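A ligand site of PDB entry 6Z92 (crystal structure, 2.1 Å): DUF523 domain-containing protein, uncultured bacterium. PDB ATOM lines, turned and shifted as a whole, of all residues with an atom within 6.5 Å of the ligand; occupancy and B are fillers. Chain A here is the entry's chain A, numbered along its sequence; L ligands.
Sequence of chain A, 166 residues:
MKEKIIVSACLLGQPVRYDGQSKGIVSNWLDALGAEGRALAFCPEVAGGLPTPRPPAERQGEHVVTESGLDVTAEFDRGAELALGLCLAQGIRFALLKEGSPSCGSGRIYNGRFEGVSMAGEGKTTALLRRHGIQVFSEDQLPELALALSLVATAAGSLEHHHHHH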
ATOM      1  N   VAL A   7      30.417 -12.489  -1.113  1.00  0.00           N
ATOM      2  CA  VAL A   7      29.042 -12.225  -0.671  1.00  0.00           C
ATOM      3  C   VAL A   7      28.951 -10.834  -0.081  1.00  0.00           C
ATOM      4  O   VAL A   7      29.834 -10.460   0.681  1.00  0.00           O
ATOM      5  CB  VAL A   7      28.582 -13.259   0.398  1.00  0.00           C
ATOM      6  CG1 VAL A   7      27.078 -13.153   0.668  1.00  0.00           C
ATOM      7  CG2 VAL A   7      28.987 -14.687   0.035  1.00  0.00           C
ATOM      8  N   SER A   8      27.842 -10.110  -0.292  1.00  0.00           N
ATOM      9  CA  SER A   8      27.608  -8.825   0.379  1.00  0.00           C
ATOM     10  C   SER A   8      27.597  -9.080   1.889  1.00  0.00           C
ATOM     11  O   SER A   8      26.869  -9.961   2.329  1.00  0.00           O
ATOM     12  CB  SER A   8      26.267  -8.234  -0.021  1.00  0.00           C
ATOM     13  OG  SER A   8      26.383  -7.563  -1.269  1.00  0.00           O
ATOM     14  N   ALA A   9      28.489  -8.402   2.637  1.00  0.00           N
ATOM     15  CA  ALA A   9      28.654  -8.599   4.090  1.00  0.00           C
ATOM     16  C   ALA A   9      27.348  -8.482   4.842  1.00  0.00           C
ATOM     17  O   ALA A   9      27.151  -9.221   5.799  1.00  0.00           O
ATOM     18  CB  ALA A   9      29.702  -7.638   4.645  1.00  0.00           C
ATOM     19  N   CYS A  10      26.441  -7.591   4.401  1.00  0.00           N
ATOM     20  CA  CYS A  10      25.146  -7.451   5.075  1.00  0.00           C
ATOM     21  C   CYS A  10      24.274  -8.716   4.932  1.00  0.00           C
ATOM     22  O   CYS A  10      23.504  -9.006   5.841  1.00  0.00           O
ATOM     23  CB  CYS A  10      24.422  -6.196   4.571  1.00  0.00           C
ATOM     24  SG  CYS A  10      24.081  -6.212   2.793  1.00  0.00           S
ATOM     25  N   LEU A  11      24.384  -9.476   3.828  1.00  0.00           N
ATOM     26  CA  LEU A  11      23.624 -10.733   3.624  1.00  0.00           C
ATOM     27  C   LEU A  11      24.027 -11.815   4.619  1.00  0.00           C
ATOM     28  O   LEU A  11      23.256 -12.739   4.876  1.00  0.00           O
ATOM     29  CB  LEU A  11      23.771 -11.278   2.201  1.00  0.00           C
ATOM     30  CG  LEU A  11      23.218 -10.398   1.069  1.00  0.00           C
ATOM     31  CD1 LEU A  11      23.533 -10.989  -0.277  1.00  0.00           C
ATOM     32  CD2 LEU A  11      21.720 -10.148   1.245  1.00  0.00           C
ATOM     33  N   GLN A  14      26.142  -9.017   8.905  1.00  0.00           N
ATOM     34  CA  GLN A  14      27.061  -7.984   9.380  1.00  0.00           C
ATOM     35  C   GLN A  14      26.461  -6.609   9.391  1.00  0.00           C
ATOM     36  O   GLN A  14      25.785  -6.218   8.438  1.00  0.00           O
ATOM     37  CB  GLN A  14      28.350  -8.021   8.598  1.00  0.00           C
ATOM     38  CG  GLN A  14      28.959  -9.389   8.812  1.00  0.00           C
ATOM     39  CD  GLN A  14      30.324  -9.491   8.284  1.00  0.00           C
ATOM     40  OE1 GLN A  14      31.064  -8.526   8.277  1.00  0.00           O
ATOM     41  NE2 GLN A  14      30.676 -10.682   7.851  1.00  0.00           N
ATOM     42  N   VAL A  16      26.999  -3.656   8.621  1.00  0.00           N
ATOM     43  CA  VAL A  16      27.687  -2.721   7.739  1.00  0.00           C
ATOM     44  C   VAL A  16      26.734  -1.919   6.838  1.00  0.00           C
ATOM     45  O   VAL A  16      27.193  -1.123   6.032  1.00  0.00           O
ATOM     46  CB  VAL A  16      28.735  -3.463   6.892  1.00  0.00           C
ATOM     47  CG1 VAL A  16      29.853  -3.987   7.784  1.00  0.00           C
ATOM     48  CG2 VAL A  16      28.089  -4.598   6.073  1.00  0.00           C
ATOM     49  N   ARG A  17      25.403  -2.117   6.972  1.00  0.00           N
ATOM     50  CA  ARG A  17      24.434  -1.350   6.188  1.00  0.00           C
ATOM     51  C   ARG A  17      24.531   0.136   6.510  1.00  0.00           C
ATOM     52  O   ARG A  17      25.022   0.493   7.579  1.00  0.00           O
ATOM     53  CB  ARG A  17      23.007  -1.840   6.473  1.00  0.00           C
ATOM     54  CG  ARG A  17      22.678  -3.203   5.852  1.00  0.00           C
ATOM     55  CD  ARG A  17      22.424  -3.090   4.339  1.00  0.00           C
ATOM     56  NE  ARG A  17      21.189  -2.373   4.035  1.00  0.00           N
ATOM     57  CZ  ARG A  17      20.624  -2.344   2.829  1.00  0.00           C
ATOM     58  NH1 ARG A  17      21.166  -3.009   1.815  1.00  0.00           N
ATOM     59  NH2 ARG A  17      19.508  -1.663   2.636  1.00  0.00           N
ATOM     60  N   TYR A  18      24.007   1.005   5.626  1.00  0.00           N
ATOM     61  CA  TYR A  18      24.077   2.448   5.850  1.00  0.00           C
ATOM     62  C   TYR A  18      23.489   2.886   7.191  1.00  0.00           C
ATOM     63  O   TYR A  18      23.936   3.874   7.754  1.00  0.00           O
ATOM     64  CB  TYR A  18      23.431   3.233   4.687  1.00  0.00           C
ATOM     65  CG  TYR A  18      21.921   3.312   4.731  1.00  0.00           C
ATOM     66  CD1 TYR A  18      21.139   2.196   4.418  1.00  0.00           C
ATOM     67  CD2 TYR A  18      21.285   4.471   5.122  1.00  0.00           C
ATOM     68  CE1 TYR A  18      19.752   2.253   4.483  1.00  0.00           C
ATOM     69  CE2 TYR A  18      19.892   4.537   5.206  1.00  0.00           C
ATOM     70  CZ  TYR A  18      19.134   3.435   4.868  1.00  0.00           C
ATOM     71  OH  TYR A  18      17.765   3.516   4.927  1.00  0.00           O
ATOM     72  N   GLN A  21      22.260  -1.491  10.445  1.00  0.00           N
ATOM     73  CA  GLN A  21      21.449  -2.681  10.520  1.00  0.00           C
ATOM     74  C   GLN A  21      22.105  -3.765   9.627  1.00  0.00           C
ATOM     75  O   GLN A  21      23.224  -3.582   9.141  1.00  0.00           O
ATOM     76  CB  GLN A  21      20.038  -2.311  10.006  1.00  0.00           C
ATOM     77  CG  GLN A  21      18.883  -3.129  10.536  1.00  0.00           C
ATOM     78  CD  GLN A  21      17.840  -3.206   9.445  1.00  0.00           C
ATOM     79  OE1 GLN A  21      17.334  -2.181   8.948  1.00  0.00           O
ATOM     80  NE2 GLN A  21      17.527  -4.430   9.017  1.00  0.00           N
ATOM     81  N   LYS A  23      21.205  -7.182   6.623  1.00  0.00           N
ATOM     82  CA  LYS A  23      20.201  -7.856   5.815  1.00  0.00           C
ATOM     83  C   LYS A  23      20.496  -9.330   5.867  1.00  0.00           C
ATOM     84  O   LYS A  23      20.649  -9.973   4.826  1.00  0.00           O
ATOM     85  CB  LYS A  23      20.216  -7.308   4.380  1.00  0.00           C
ATOM     86  CG  LYS A  23      19.801  -5.853   4.326  1.00  0.00           C
ATOM     87  CD  LYS A  23      18.326  -5.643   4.687  1.00  0.00           C
ATOM     88  CE  LYS A  23      18.082  -4.329   5.389  1.00  0.00           C
ATOM     89  NZ  LYS A  23      17.047  -3.513   4.697  1.00  0.00           N
ATOM     90  N   PHE A  42      32.116  -9.366   2.028  1.00  0.00           N
ATOM     91  CA  PHE A  42      32.674  -8.155   1.462  1.00  0.00           C
ATOM     92  C   PHE A  42      31.649  -7.027   1.418  1.00  0.00           C
ATOM     93  O   PHE A  42      30.527  -7.242   0.987  1.00  0.00           O
ATOM     94  CB  PHE A  42      33.237  -8.403   0.045  1.00  0.00           C
ATOM     95  CG  PHE A  42      34.044  -7.245  -0.490  1.00  0.00           C
ATOM     96  CD1 PHE A  42      33.463  -6.315  -1.340  1.00  0.00           C
ATOM     97  CD2 PHE A  42      35.348  -7.041  -0.089  1.00  0.00           C
ATOM     98  CE1 PHE A  42      34.176  -5.214  -1.762  1.00  0.00           C
ATOM     99  CE2 PHE A  42      36.056  -5.951  -0.532  1.00  0.00           C
ATOM    100  CZ  PHE A  42      35.473  -5.042  -1.353  1.00  0.00           C
ATOM    101  N   CYS A  43      32.049  -5.831   1.840  1.00  0.00           N
ATOM    102  CA  CYS A  43      31.187  -4.666   1.714  1.00  0.00           C
ATOM    103  C   CYS A  43      31.919  -3.625   0.897  1.00  0.00           C
ATOM    104  O   CYS A  43      32.859  -3.034   1.395  1.00  0.00           O
ATOM    105  CB  CYS A  43      30.752  -4.114   3.077  1.00  0.00           C
ATOM    106  SG  CYS A  43      29.766  -2.604   2.956  1.00  0.00           S
ATOM    107  N   PRO A  44      31.486  -3.352  -0.335  1.00  0.00           N
ATOM    108  CA  PRO A  44      32.123  -2.306  -1.139  1.00  0.00           C
ATOM    109  C   PRO A  44      32.181  -0.913  -0.523  1.00  0.00           C
ATOM    110  O   PRO A  44      33.170  -0.209  -0.723  1.00  0.00           O
ATOM    111  CB  PRO A  44      31.261  -2.281  -2.407  1.00  0.00           C
ATOM    112  CG  PRO A  44      30.689  -3.622  -2.500  1.00  0.00           C
ATOM    113  CD  PRO A  44      30.383  -3.993  -1.078  1.00  0.00           C
ATOM    114  N   GLU A  45      31.144  -0.491   0.189  1.00  0.00           N
ATOM    115  CA  GLU A  45      31.087   0.855   0.742  1.00  0.00           C
ATOM    116  C   GLU A  45      32.019   1.015   1.919  1.00  0.00           C
ATOM    117  O   GLU A  45      32.739   2.015   1.992  1.00  0.00           O
ATOM    118  CB  GLU A  45      29.645   1.243   1.057  1.00  0.00           C
ATOM    119  CG  GLU A  45      28.898   1.438  -0.244  1.00  0.00           C
ATOM    120  CD  GLU A  45      27.390   1.536  -0.117  1.00  0.00           C
ATOM    121  OE1 GLU A  45      26.935   2.113   0.887  1.00  0.00           O
ATOM    122  OE2 GLU A  45      26.673   1.060  -1.028  1.00  0.00           O
ATOM    123  N   VAL A  46      32.072   0.013   2.795  1.00  0.00           N
ATOM    124  CA  VAL A  46      33.001   0.052   3.926  1.00  0.00           C
ATOM    125  C   VAL A  46      34.446  -0.139   3.428  1.00  0.00           C
ATOM    126  O   VAL A  46      35.355   0.569   3.886  1.00  0.00           O
ATOM    127  CB  VAL A  46      32.597  -0.974   5.015  1.00  0.00           C
ATOM    128  CG1 VAL A  46      33.698  -1.129   6.034  1.00  0.00           C
ATOM    129  CG2 VAL A  46      31.298  -0.552   5.702  1.00  0.00           C
ATOM    130  N   ARG A  54      26.067   5.878   7.543  1.00  0.00           N
ATOM    131  CA  ARG A  54      26.363   6.807   6.450  1.00  0.00           C
ATOM    132  C   ARG A  54      25.049   7.144   5.768  1.00  0.00           C
ATOM    133  O   ARG A  54      24.092   6.358   5.806  1.00  0.00           O
ATOM    134  CB  ARG A  54      27.369   6.184   5.448  1.00  0.00           C
ATOM    135  CG  ARG A  54      26.879   4.887   4.812  1.00  0.00           C
ATOM    136  CD  ARG A  54      27.959   4.210   4.013  1.00  0.00           C
ATOM    137  NE  ARG A  54      27.528   2.909   3.510  1.00  0.00           N
ATOM    138  CZ  ARG A  54      27.612   1.774   4.212  1.00  0.00           C
ATOM    139  NH1 ARG A  54      28.105   1.784   5.447  1.00  0.00           N
ATOM    140  NH2 ARG A  54      27.183   0.625   3.685  1.00  0.00           N
ATOM    141  N   PHE A  76      32.733   4.505  -3.856  1.00  0.00           N
ATOM    142  CA  PHE A  76      31.976   3.450  -4.527  1.00  0.00           C
ATOM    143  C   PHE A  76      32.845   2.705  -5.518  1.00  0.00           C
ATOM    144  O   PHE A  76      32.838   1.479  -5.538  1.00  0.00           O
ATOM    145  CB  PHE A  76      30.728   4.031  -5.206  1.00  0.00           C
ATOM    146  CG  PHE A  76      29.535   4.059  -4.265  1.00  0.00           C
ATOM    147  CD1 PHE A  76      29.486   4.941  -3.205  1.00  0.00           C
ATOM    148  CD2 PHE A  76      28.488   3.172  -4.441  1.00  0.00           C
ATOM    149  CE1 PHE A  76      28.400   4.947  -2.328  1.00  0.00           C
ATOM    150  CE2 PHE A  76      27.381   3.196  -3.577  1.00  0.00           C
ATOM    151  CZ  PHE A  76      27.355   4.081  -2.532  1.00  0.00           C
ATOM    152  N   LEU A  97      25.245 -10.713  -4.252  1.00  0.00           N
ATOM    153  CA  LEU A  97      25.158  -9.329  -3.795  1.00  0.00           C
ATOM    154  C   LEU A  97      23.740  -8.866  -3.503  1.00  0.00           C
ATOM    155  O   LEU A  97      22.792  -9.282  -4.157  1.00  0.00           O
ATOM    156  CB  LEU A  97      25.857  -8.390  -4.796  1.00  0.00           C
ATOM    157  CG  LEU A  97      27.304  -8.746  -5.169  1.00  0.00           C
ATOM    158  CD1 LEU A  97      27.868  -7.737  -6.160  1.00  0.00           C
ATOM    159  CD2 LEU A  97      28.208  -8.804  -3.936  1.00  0.00           C
ATOM    160  N   LYS A  98      23.600  -7.957  -2.528  1.00  0.00           N
ATOM    161  CA  LYS A  98      22.358  -7.369  -2.067  1.00  0.00           C
ATOM    162  C   LYS A  98      21.587  -6.545  -3.139  1.00  0.00           C
ATOM    163  O   LYS A  98      22.101  -5.563  -3.672  1.00  0.00           O
ATOM    164  CB  LYS A  98      22.649  -6.499  -0.836  1.00  0.00           C
ATOM    165  CG  LYS A  98      21.422  -5.810  -0.256  1.00  0.00           C
ATOM    166  CD  LYS A  98      20.471  -6.801   0.424  1.00  0.00           C
ATOM    167  CE  LYS A  98      19.112  -6.216   0.630  1.00  0.00           C
ATOM    168  NZ  LYS A  98      18.306  -6.163  -0.626  1.00  0.00           N
ATOM    169  N   GLU A  99      20.350  -6.922  -3.425  1.00  0.00           N
ATOM    170  CA  GLU A  99      19.498  -6.234  -4.395  1.00  0.00           C
ATOM    171  C   GLU A  99      19.104  -4.795  -3.988  1.00  0.00           C
ATOM    172  O   GLU A  99      18.975  -4.506  -2.788  1.00  0.00           O
ATOM    173  CB  GLU A  99      18.253  -7.079  -4.644  1.00  0.00           C
ATOM    174  CG  GLU A  99      17.406  -6.639  -5.828  1.00  0.00           C
ATOM    175  CD  GLU A  99      18.157  -6.627  -7.139  1.00  0.00           C
ATOM    176  OE1 GLU A  99      18.917  -5.654  -7.376  1.00  0.00           O
ATOM    177  OE2 GLU A  99      17.963  -7.561  -7.950  1.00  0.00           O
ATOM    178  N   SER A 101      20.786  -2.033  -4.110  1.00  0.00           N
ATOM    179  CA  SER A 101      21.911  -1.232  -3.620  1.00  0.00           C
ATOM    180  C   SER A 101      22.652  -0.476  -4.755  1.00  0.00           C
ATOM    181  O   SER A 101      22.883  -1.025  -5.848  1.00  0.00           O
ATOM    182  CB  SER A 101      22.858  -2.134  -2.826  1.00  0.00           C
ATOM    183  OG  SER A 101      24.145  -1.575  -2.625  1.00  0.00           O
ATOM    184  N   PRO A 102      23.051   0.785  -4.492  1.00  0.00           N
ATOM    185  CA  PRO A 102      23.855   1.496  -5.486  1.00  0.00           C
ATOM    186  C   PRO A 102      25.251   0.877  -5.698  1.00  0.00           C
ATOM    187  O   PRO A 102      25.968   1.260  -6.621  1.00  0.00           O
ATOM    188  CB  PRO A 102      23.920   2.922  -4.939  1.00  0.00           C
ATOM    189  CG  PRO A 102      23.761   2.775  -3.439  1.00  0.00           C
ATOM    190  CD  PRO A 102      22.900   1.555  -3.232  1.00  0.00           C
ATOM    191  N   SER A 103      25.619  -0.116  -4.868  1.00  0.00           N
ATOM    192  CA  SER A 103      26.863  -0.853  -4.939  1.00  0.00           C
ATOM    193  C   SER A 103      26.585  -2.293  -5.433  1.00  0.00           C
ATOM    194  O   SER A 103      27.142  -2.722  -6.443  1.00  0.00           O
ATOM    195  CB  SER A 103      27.507  -0.945  -3.550  1.00  0.00           C
ATOM    196  OG  SER A 103      28.355   0.141  -3.237  1.00  0.00           O
ATOM    197  N   CYS A 104      25.691  -3.023  -4.720  1.00  0.00           N
ATOM    198  CA  CYS A 104      25.410  -4.440  -4.878  1.00  0.00           C
ATOM    199  C   CYS A 104      24.173  -4.826  -5.723  1.00  0.00           C
ATOM    200  O   CYS A 104      23.988  -6.012  -6.036  1.00  0.00           O
ATOM    201  CB  CYS A 104      25.347  -5.085  -3.497  1.00  0.00           C
ATOM    202  SG  CYS A 104      26.852  -4.873  -2.512  1.00  0.00           S
ATOM    203  N   GLY A 105      23.305  -3.850  -6.052  1.00  0.00           N
ATOM    204  CA  GLY A 105      22.113  -4.119  -6.843  1.00  0.00           C
ATOM    205  C   GLY A 105      22.425  -4.771  -8.182  1.00  0.00           C
ATOM    206  O   GLY A 105      23.407  -4.384  -8.814  1.00  0.00           O
HETATM  207 FE1  LIG L   1      25.472  -1.907   1.302  1.00  0.00          FE
HETATM  208 FE2  LIG L   1      25.417  -4.641   1.944  1.00  0.00          FE
HETATM  209 FE3  LIG L   1      27.787  -3.223   1.980  1.00  0.00          FE
HETATM  210 FE4  LIG L   1      26.522  -3.784  -0.423  1.00  0.00          FE
HETATM  211  S1  LIG L   1      27.441  -5.303   1.088  1.00  0.00           S
HETATM  212  S2  LIG L   1      27.465  -1.749   0.216  1.00  0.00           S
HETATM  213  S3  LIG L   1      24.338  -3.577   0.169  1.00  0.00           S
HETATM  214  S4  LIG L   1      25.979  -2.904   3.345  1.00  0.00           S
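The guanidinium group (NH1) of Arg 17 sits close to a sulfur (S3) of the ligand (3.6 Å). A sulfur (S4) of the ligand sits close to the backbone NH (N) of Arg 17. S4 of the ligand lies close to NH2 of Arg 54, 3.7 Å away. The side-chain sulfur (SG) of Cys 10 is bound to an iron atom (FE2) of the ligand (2.2 Å). The side-chain hydroxyl (OG) of Ser 101 sits close to a sulfur (S3) of the ligand, 3.4 Å away. FE4 of the ligand is bound by SG of Cys 104 (2.4 Å). A sulfur (S1) of the ligand sits close to the side-chain hydroxyl of Ser 8. The backbone NH of Ala 9 lies close to a sulfur (S1) of the ligand (3.6 Å). SG of Cys 43 binds FE3 of the ligand (2.3 Å).
SG of Cys 43 lies close to N of Glu 45 (3.7 Å). The backbone carbonyl oxygen (O) of Lys 98 sits at hydrogen-bond distance from the backbone NH (N) of Gly 105. OG of Ser 8 lies within hydrogen-bond range of N of Lys 98, at 3.1 Å. The backbone NH (N) of Ser 103 lies close to the side-chain hydroxyl (OG) of Ser 101 (3.1 Å). The side-chain sulfur (SG) of Cys 104 lies close to the side-chain hydroxyl (OG) of Ser 8 (3.0 Å). The backbone NH (N) of Phe 42 is in hydrogen-bond range of the backbone carbonyl oxygen (O) of Val 7 (2.9 Å). The backbone NH (N) of Arg 54 lies within hydrogen-bond range of the backbone carbonyl oxygen (O) of Tyr 18 (2.9 Å). The side-chain carboxylate (OE2) of Glu 45 sits at hydrogen-bond distance from the side-chain hydroxyl (OG) of Ser 103 (2.9 Å).
A sulfur (S4) of the ligand lies close to the backbone carbonyl oxygen (O) of Val 16. The backbone carbonyl oxygen of Phe 42 sits close to a sulfur (S1) of the ligand. A sulfur (S2) of the ligand lies close to the side-chain carboxylate (OE2) of Glu 45, at 3.2 Å. Pro 44 touches the ligand (CD to S1, 3.9 Å). Lys 98 touches the ligand. Ser 103 touches the ligand. Of the 26 residues printed, 14 come within 4 Å of the ligand. The nearest printed residue that does not touch the ligand is Tyr 18 (4.9 Å).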
